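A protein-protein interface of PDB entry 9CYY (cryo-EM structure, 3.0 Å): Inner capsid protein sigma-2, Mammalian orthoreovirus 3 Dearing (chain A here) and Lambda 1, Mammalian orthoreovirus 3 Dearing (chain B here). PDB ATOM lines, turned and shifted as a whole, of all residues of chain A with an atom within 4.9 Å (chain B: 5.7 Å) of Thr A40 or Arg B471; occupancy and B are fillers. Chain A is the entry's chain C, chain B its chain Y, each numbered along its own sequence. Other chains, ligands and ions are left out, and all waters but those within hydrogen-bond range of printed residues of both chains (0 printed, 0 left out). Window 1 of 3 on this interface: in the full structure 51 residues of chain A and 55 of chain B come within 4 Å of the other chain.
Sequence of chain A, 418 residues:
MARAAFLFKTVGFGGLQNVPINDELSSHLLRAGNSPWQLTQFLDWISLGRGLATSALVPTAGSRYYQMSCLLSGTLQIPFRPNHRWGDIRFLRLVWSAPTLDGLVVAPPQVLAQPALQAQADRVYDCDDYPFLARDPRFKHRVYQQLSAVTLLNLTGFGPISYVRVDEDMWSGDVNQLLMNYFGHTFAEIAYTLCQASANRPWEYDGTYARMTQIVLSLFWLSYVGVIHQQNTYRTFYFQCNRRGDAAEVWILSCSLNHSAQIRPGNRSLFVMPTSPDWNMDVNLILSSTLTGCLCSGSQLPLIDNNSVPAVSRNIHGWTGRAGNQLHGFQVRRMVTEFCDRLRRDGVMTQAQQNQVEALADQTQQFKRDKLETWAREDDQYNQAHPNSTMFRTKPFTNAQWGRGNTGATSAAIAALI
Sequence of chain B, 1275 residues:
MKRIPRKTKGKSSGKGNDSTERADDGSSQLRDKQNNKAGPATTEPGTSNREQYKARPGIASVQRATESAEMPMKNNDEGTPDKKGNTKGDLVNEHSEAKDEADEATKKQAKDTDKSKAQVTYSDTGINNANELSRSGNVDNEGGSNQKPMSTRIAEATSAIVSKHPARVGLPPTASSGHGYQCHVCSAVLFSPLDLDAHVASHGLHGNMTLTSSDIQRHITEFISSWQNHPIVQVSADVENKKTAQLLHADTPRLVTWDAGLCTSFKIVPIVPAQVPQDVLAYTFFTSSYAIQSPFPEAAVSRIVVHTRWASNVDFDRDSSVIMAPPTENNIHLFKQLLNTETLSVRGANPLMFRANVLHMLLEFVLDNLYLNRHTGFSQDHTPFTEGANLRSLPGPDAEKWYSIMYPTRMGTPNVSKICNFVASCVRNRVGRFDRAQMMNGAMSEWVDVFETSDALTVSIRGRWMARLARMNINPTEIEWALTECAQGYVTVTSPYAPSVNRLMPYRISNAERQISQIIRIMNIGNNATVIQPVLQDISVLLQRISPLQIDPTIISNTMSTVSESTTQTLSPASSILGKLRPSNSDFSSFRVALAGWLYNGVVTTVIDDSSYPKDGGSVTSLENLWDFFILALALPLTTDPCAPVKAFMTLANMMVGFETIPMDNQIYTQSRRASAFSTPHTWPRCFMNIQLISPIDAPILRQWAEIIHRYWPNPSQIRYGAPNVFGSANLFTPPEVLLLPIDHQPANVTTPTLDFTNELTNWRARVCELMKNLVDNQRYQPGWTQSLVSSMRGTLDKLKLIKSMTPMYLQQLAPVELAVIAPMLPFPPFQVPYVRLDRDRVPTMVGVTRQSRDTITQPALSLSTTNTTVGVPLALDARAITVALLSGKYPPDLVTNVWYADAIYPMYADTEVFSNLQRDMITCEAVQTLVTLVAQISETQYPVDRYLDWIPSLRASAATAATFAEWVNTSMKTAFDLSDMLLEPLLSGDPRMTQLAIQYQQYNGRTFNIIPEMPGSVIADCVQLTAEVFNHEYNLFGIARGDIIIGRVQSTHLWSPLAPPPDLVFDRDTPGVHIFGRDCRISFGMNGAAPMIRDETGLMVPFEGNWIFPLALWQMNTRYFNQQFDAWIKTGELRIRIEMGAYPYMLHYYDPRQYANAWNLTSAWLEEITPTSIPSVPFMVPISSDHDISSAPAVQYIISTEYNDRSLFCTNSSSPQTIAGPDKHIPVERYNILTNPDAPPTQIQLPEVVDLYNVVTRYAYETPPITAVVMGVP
The side-chain carboxylate of Asp A44 lies within salt-bridge range of the guanidinium group of Arg B471 (2.4 Å). OE1 of Gln A196 sits at hydrogen-bond distance from NE of Arg B471 (3.3 Å).
Of the 9 printed residues of chain A, 5 touch a printed residue of chain B. Hydrophobic or aromatic side chains of chain A within 4 Å of the printed part of chain B: Tyr A192. Of the 11 printed residues of chain B, 5 touch a printed residue of chain A.
Among the printed residues, merely in contact across the chains: Gln A196 with Arg B508 (3.6 Å), Asp A44 with Arg B468 (3.6 Å), Thr A40 with Arg B471 (3.9 Å), Gln A41 with Gly B1017 (3.9 Å) and Tyr A192 with Ala B467 (3.98 Å).
Of the printed residues of chain B, Gln A41 touches Gly B1017. Of the printed residues of chain B, Asp A44 touches Arg B468 and Arg B471. Printed residues of chain B within 4 Å of Gln A196: Arg B471 and Arg B508. Leu B469 touches none of the printed residues of chain A. Arg B471 touches just these residues of chain A: Thr A40 (3.9 Å), Asp A44 (2.4 Å) and Gln A196 (3.3 Å). Met B472 touches none of the printed residues of chain A. Of the printed residues of chain A, Arg B508 touches Gln A196. The nearest residue of chain B that does not touch Thr A40 is Gly B1017 (5.1 Å).
NE2 of Gln A38 sits close to NE2 of Gln A41, at 3.3 Å. The side-chain hydroxyl (OH) of Tyr A192 sits at hydrogen-bond distance from the backbone carbonyl oxygen (O) of Leu A43 (2.4 Å). The side-chain sulfur of Met B472 sits close to the guanidinium group of Arg B468. NH2 of Arg B468 lies within salt-bridge range of OE2 of Glu B513 (3.6 Å). The backbone carbonyl oxygen of Met B472 sits at hydrogen-bond distance from the backbone NH of Arg B508, 3.4 Å away.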
ATOM      1  N   GLN A  38     -24.539  -3.387   1.390  1.00  0.00           N
ATOM      2  CA  GLN A  38     -23.867  -2.844   2.564  1.00  0.00           C
ATOM      3  C   GLN A  38     -23.156  -1.537   2.248  1.00  0.00           C
ATOM      4  O   GLN A  38     -22.108  -1.227   2.822  1.00  0.00           O
ATOM      5  CB  GLN A  38     -22.878  -3.858   3.132  1.00  0.00           C
ATOM      6  CG  GLN A  38     -23.533  -5.052   3.786  1.00  0.00           C
ATOM      7  CD  GLN A  38     -22.725  -5.584   4.944  1.00  0.00           C
ATOM      8  OE1 GLN A  38     -21.506  -5.428   4.987  1.00  0.00           O
ATOM      9  NE2 GLN A  38     -23.399  -6.217   5.894  1.00  0.00           N
ATOM     10  N   LEU A  39     -23.715  -0.741   1.339  1.00  0.00           N
ATOM     11  CA  LEU A  39     -23.083   0.528   0.994  1.00  0.00           C
ATOM     12  C   LEU A  39     -23.092   1.493   2.176  1.00  0.00           C
ATOM     13  O   LEU A  39     -22.072   2.126   2.478  1.00  0.00           O
ATOM     14  CB  LEU A  39     -23.784   1.139  -0.216  1.00  0.00           C
ATOM     15  CG  LEU A  39     -23.010   2.211  -0.977  1.00  0.00           C
ATOM     16  CD1 LEU A  39     -21.675   1.658  -1.430  1.00  0.00           C
ATOM     17  CD2 LEU A  39     -23.821   2.670  -2.169  1.00  0.00           C
ATOM     18  N   THR A  40     -24.230   1.609   2.863  1.00  0.00           N
ATOM     19  CA  THR A  40     -24.315   2.496   4.018  1.00  0.00           C
ATOM     20  C   THR A  40     -23.420   2.010   5.152  1.00  0.00           C
ATOM     21  O   THR A  40     -22.789   2.812   5.851  1.00  0.00           O
ATOM     22  CB  THR A  40     -25.764   2.606   4.486  1.00  0.00           C
ATOM     23  OG1 THR A  40     -26.329   1.294   4.599  1.00  0.00           O
ATOM     24  CG2 THR A  40     -26.578   3.413   3.492  1.00  0.00           C
ATOM     25  N   GLN A  41     -23.363   0.693   5.356  1.00  0.00           N
ATOM     26  CA  GLN A  41     -22.488   0.146   6.385  1.00  0.00           C
ATOM     27  C   GLN A  41     -21.026   0.433   6.070  1.00  0.00           C
ATOM     28  O   GLN A  41     -20.241   0.750   6.968  1.00  0.00           O
ATOM     29  CB  GLN A  41     -22.729  -1.355   6.529  1.00  0.00           C
ATOM     30  CG  GLN A  41     -24.197  -1.734   6.552  1.00  0.00           C
ATOM     31  CD  GLN A  41     -24.482  -2.915   7.453  1.00  0.00           C
ATOM     32  OE1 GLN A  41     -23.920  -3.030   8.541  1.00  0.00           O
ATOM     33  NE2 GLN A  41     -25.362  -3.802   7.005  1.00  0.00           N
ATOM     34  N   PHE A  42     -20.644   0.329   4.795  1.00  0.00           N
ATOM     35  CA  PHE A  42     -19.284   0.672   4.394  1.00  0.00           C
ATOM     36  C   PHE A  42     -18.994   2.148   4.638  1.00  0.00           C
ATOM     37  O   PHE A  42     -17.905   2.514   5.105  1.00  0.00           O
ATOM     38  CB  PHE A  42     -19.084   0.313   2.922  1.00  0.00           C
ATOM     39  CG  PHE A  42     -17.800   0.817   2.337  1.00  0.00           C
ATOM     40  CD1 PHE A  42     -16.595   0.235   2.677  1.00  0.00           C
ATOM     41  CD2 PHE A  42     -17.801   1.866   1.436  1.00  0.00           C
ATOM     42  CE1 PHE A  42     -15.414   0.691   2.133  1.00  0.00           C
ATOM     43  CE2 PHE A  42     -16.624   2.327   0.892  1.00  0.00           C
ATOM     44  CZ  PHE A  42     -15.429   1.739   1.241  1.00  0.00           C
ATOM     45  N   LEU A  43     -19.962   3.013   4.322  1.00  0.00           N
ATOM     46  CA  LEU A  43     -19.793   4.442   4.564  1.00  0.00           C
ATOM     47  C   LEU A  43     -19.592   4.729   6.046  1.00  0.00           C
ATOM     48  O   LEU A  43     -18.749   5.551   6.419  1.00  0.00           O
ATOM     49  CB  LEU A  43     -21.001   5.213   4.036  1.00  0.00           C
ATOM     50  CG  LEU A  43     -21.144   5.343   2.522  1.00  0.00           C
ATOM     51  CD1 LEU A  43     -22.295   6.269   2.182  1.00  0.00           C
ATOM     52  CD2 LEU A  43     -19.854   5.845   1.906  1.00  0.00           C
ATOM     53  N   ASP A  44     -20.372   4.071   6.905  1.00  0.00           N
ATOM     54  CA  ASP A  44     -20.187   4.244   8.342  1.00  0.00           C
ATOM     55  C   ASP A  44     -18.836   3.708   8.799  1.00  0.00           C
ATOM     56  O   ASP A  44     -18.175   4.319   9.647  1.00  0.00           O
ATOM     57  CB  ASP A  44     -21.317   3.558   9.106  1.00  0.00           C
ATOM     58  CG  ASP A  44     -22.674   4.151   8.794  1.00  0.00           C
ATOM     59  OD1 ASP A  44     -22.771   4.935   7.828  1.00  0.00           O
ATOM     60  OD2 ASP A  44     -23.644   3.833   9.513  1.00  0.00           O
ATOM     61  N   TYR A 192     -21.105  11.422   0.790  1.00  0.00           N
ATOM     62  CA  TYR A 192     -22.085  10.821   1.689  1.00  0.00           C
ATOM     63  C   TYR A 192     -23.490  11.324   1.385  1.00  0.00           C
ATOM     64  O   TYR A 192     -24.424  10.531   1.195  1.00  0.00           O
ATOM     65  CB  TYR A 192     -21.724  11.130   3.142  1.00  0.00           C
ATOM     66  CG  TYR A 192     -20.718  10.199   3.777  1.00  0.00           C
ATOM     67  CD1 TYR A 192     -19.656   9.683   3.052  1.00  0.00           C
ATOM     68  CD2 TYR A 192     -20.824   9.852   5.114  1.00  0.00           C
ATOM     69  CE1 TYR A 192     -18.734   8.842   3.639  1.00  0.00           C
ATOM     70  CE2 TYR A 192     -19.910   9.012   5.708  1.00  0.00           C
ATOM     71  CZ  TYR A 192     -18.868   8.511   4.968  1.00  0.00           C
ATOM     72  OH  TYR A 192     -17.957   7.673   5.562  1.00  0.00           O
ATOM     73  N   GLN A 196     -26.588   9.096  -0.265  1.00  0.00           N
ATOM     74  CA  GLN A 196     -27.845   8.893   0.450  1.00  0.00           C
ATOM     75  C   GLN A 196     -29.033   9.387  -0.367  1.00  0.00           C
ATOM     76  O   GLN A 196     -30.082   8.730  -0.415  1.00  0.00           O
ATOM     77  CB  GLN A 196     -27.800   9.582   1.811  1.00  0.00           C
ATOM     78  CG  GLN A 196     -29.109   9.497   2.571  1.00  0.00           C
ATOM     79  CD  GLN A 196     -29.388   8.106   3.095  1.00  0.00           C
ATOM     80  OE1 GLN A 196     -28.735   7.637   4.025  1.00  0.00           O
ATOM     81  NE2 GLN A 196     -30.359   7.432   2.493  1.00  0.00           N
ATOM     82  N   MET B 466     -20.023  10.473  14.288  1.00  0.00           N
ATOM     83  CA  MET B 466     -19.999  11.659  13.441  1.00  0.00           C
ATOM     84  C   MET B 466     -20.285  11.303  11.990  1.00  0.00           C
ATOM     85  O   MET B 466     -20.985  12.041  11.291  1.00  0.00           O
ATOM     86  CB  MET B 466     -18.651  12.365  13.569  1.00  0.00           C
ATOM     87  CG  MET B 466     -18.470  13.522  12.608  1.00  0.00           C
ATOM     88  SD  MET B 466     -19.475  14.944  13.071  1.00  0.00           S
ATOM     89  CE  MET B 466     -19.855  15.630  11.464  1.00  0.00           C
ATOM     90  N   ALA B 467     -19.748  10.176  11.515  1.00  0.00           N
ATOM     91  CA  ALA B 467     -20.027   9.747  10.147  1.00  0.00           C
ATOM     92  C   ALA B 467     -21.510   9.452   9.958  1.00  0.00           C
ATOM     93  O   ALA B 467     -22.105   9.805   8.930  1.00  0.00           O
ATOM     94  CB  ALA B 467     -19.183   8.520   9.803  1.00  0.00           C
ATOM     95  N   ARG B 468     -22.125   8.802  10.948  1.00  0.00           N
ATOM     96  CA  ARG B 468     -23.550   8.508  10.858  1.00  0.00           C
ATOM     97  C   ARG B 468     -24.372   9.786  10.771  1.00  0.00           C
ATOM     98  O   ARG B 468     -25.317   9.872   9.979  1.00  0.00           O
ATOM     99  CB  ARG B 468     -23.995   7.673  12.056  1.00  0.00           C
ATOM    100  CG  ARG B 468     -25.481   7.379  12.068  1.00  0.00           C
ATOM    101  CD  ARG B 468     -25.803   6.181  11.194  1.00  0.00           C
ATOM    102  NE  ARG B 468     -27.237   6.006  11.001  1.00  0.00           N
ATOM    103  CZ  ARG B 468     -27.992   6.784  10.241  1.00  0.00           C
ATOM    104  NH1 ARG B 468     -27.477   7.794   9.560  1.00  0.00           N
ATOM    105  NH2 ARG B 468     -29.296   6.539  10.153  1.00  0.00           N
ATOM    106  N   LEU B 469     -24.032  10.792  11.580  1.00  0.00           N
ATOM    107  CA  LEU B 469     -24.760  12.060  11.504  1.00  0.00           C
ATOM    108  C   LEU B 469     -24.510  12.769  10.174  1.00  0.00           C
ATOM    109  O   LEU B 469     -25.428  13.364   9.587  1.00  0.00           O
ATOM    110  CB  LEU B 469     -24.373  12.960  12.675  1.00  0.00           C
ATOM    111  CG  LEU B 469     -24.764  12.445  14.060  1.00  0.00           C
ATOM    112  CD1 LEU B 469     -24.339  13.429  15.133  1.00  0.00           C
ATOM    113  CD2 LEU B 469     -26.257  12.188  14.130  1.00  0.00           C
ATOM    114  N   ALA B 470     -23.269  12.719   9.684  1.00  0.00           N
ATOM    115  CA  ALA B 470     -22.941  13.366   8.421  1.00  0.00           C
ATOM    116  C   ALA B 470     -23.732  12.762   7.274  1.00  0.00           C
ATOM    117  O   ALA B 470     -24.107  13.466   6.330  1.00  0.00           O
ATOM    118  CB  ALA B 470     -21.441  13.265   8.153  1.00  0.00           C
ATOM    119  N   ARG B 471     -23.995  11.454   7.330  1.00  0.00           N
ATOM    120  CA  ARG B 471     -24.831  10.855   6.297  1.00  0.00           C
ATOM    121  C   ARG B 471     -26.267  11.364   6.356  1.00  0.00           C
ATOM    122  O   ARG B 471     -27.001  11.228   5.373  1.00  0.00           O
ATOM    123  CB  ARG B 471     -24.819   9.330   6.402  1.00  0.00           C
ATOM    124  CG  ARG B 471     -25.131   8.644   5.081  1.00  0.00           C
ATOM    125  CD  ARG B 471     -25.022   7.134   5.168  1.00  0.00           C
ATOM    126  NE  ARG B 471     -26.200   6.532   5.780  1.00  0.00           N
ATOM    127  CZ  ARG B 471     -26.191   5.862   6.923  1.00  0.00           C
ATOM    128  NH1 ARG B 471     -25.079   5.696   7.616  1.00  0.00           N
ATOM    129  NH2 ARG B 471     -27.327   5.344   7.379  1.00  0.00           N
ATOM    130  N   MET B 472     -26.680  11.948   7.478  1.00  0.00           N
ATOM    131  CA  MET B 472     -28.023  12.489   7.641  1.00  0.00           C
ATOM    132  C   MET B 472     -28.107  13.982   7.361  1.00  0.00           C
ATOM    133  O   MET B 472     -29.212  14.497   7.168  1.00  0.00           O
ATOM    134  CB  MET B 472     -28.535  12.217   9.058  1.00  0.00           C
ATOM    135  CG  MET B 472     -28.768  10.759   9.377  1.00  0.00           C
ATOM    136  SD  MET B 472     -29.287  10.520  11.087  1.00  0.00           S
ATOM    137  CE  MET B 472     -30.936  11.206  11.040  1.00  0.00           C
ATOM    138  N   ASN B 473     -26.979  14.689   7.353  1.00  0.00           N
ATOM    139  CA  ASN B 473     -26.997  16.134   7.139  1.00  0.00           C
ATOM    140  C   ASN B 473     -27.667  16.511   5.818  1.00  0.00           C
ATOM    141  O   ASN B 473     -27.523  15.816   4.809  1.00  0.00           O
ATOM    142  CB  ASN B 473     -25.572  16.684   7.162  1.00  0.00           C
ATOM    143  CG  ASN B 473     -25.529  18.179   7.390  1.00  0.00           C
ATOM    144  OD1 ASN B 473     -26.530  18.873   7.230  1.00  0.00           O
ATOM    145  ND2 ASN B 473     -24.361  18.685   7.760  1.00  0.00           N
ATOM    146  N   ARG B 508     -32.367  13.329   7.277  1.00  0.00           N
ATOM    147  CA  ARG B 508     -32.687  12.437   6.169  1.00  0.00           C
ATOM    148  C   ARG B 508     -32.429  10.991   6.568  1.00  0.00           C
ATOM    149  O   ARG B 508     -31.327  10.650   7.008  1.00  0.00           O
ATOM    150  CB  ARG B 508     -31.873  12.798   4.926  1.00  0.00           C
ATOM    151  CG  ARG B 508     -32.194  11.947   3.713  1.00  0.00           C
ATOM    152  CD  ARG B 508     -31.322  12.322   2.531  1.00  0.00           C
ATOM    153  NE  ARG B 508     -31.734  13.578   1.919  1.00  0.00           N
ATOM    154  CZ  ARG B 508     -30.993  14.273   1.068  1.00  0.00           C
ATOM    155  NH1 ARG B 508     -29.785  13.870   0.715  1.00  0.00           N
ATOM    156  NH2 ARG B 508     -31.476  15.400   0.557  1.00  0.00           N
ATOM    157  N   GLU B 513     -36.342   2.473   7.052  1.00  0.00           N
ATOM    158  CA  GLU B 513     -36.626   2.939   8.404  1.00  0.00           C
ATOM    159  C   GLU B 513     -38.048   3.472   8.513  1.00  0.00           C
ATOM    160  O   GLU B 513     -38.754   3.186   9.491  1.00  0.00           O
ATOM    161  CB  GLU B 513     -35.616   4.010   8.811  1.00  0.00           C
ATOM    162  CG  GLU B 513     -34.250   3.455   9.166  1.00  0.00           C
ATOM    163  CD  GLU B 513     -33.127   4.414   8.838  1.00  0.00           C
ATOM    164  OE1 GLU B 513     -33.043   4.859   7.676  1.00  0.00           O
ATOM    165  OE2 GLU B 513     -32.323   4.720   9.742  1.00  0.00           O
ATOM    166  N   GLY B1017     -28.303  -1.038   8.698  1.00  0.00           N
ATOM    167  CA  GLY B1017     -27.290  -1.289   9.701  1.00  0.00           C
ATOM    168  C   GLY B1017     -27.514  -0.487  10.968  1.00  0.00           C
ATOM    169  O   GLY B1017     -28.375   0.388  11.056  1.00  0.00           O
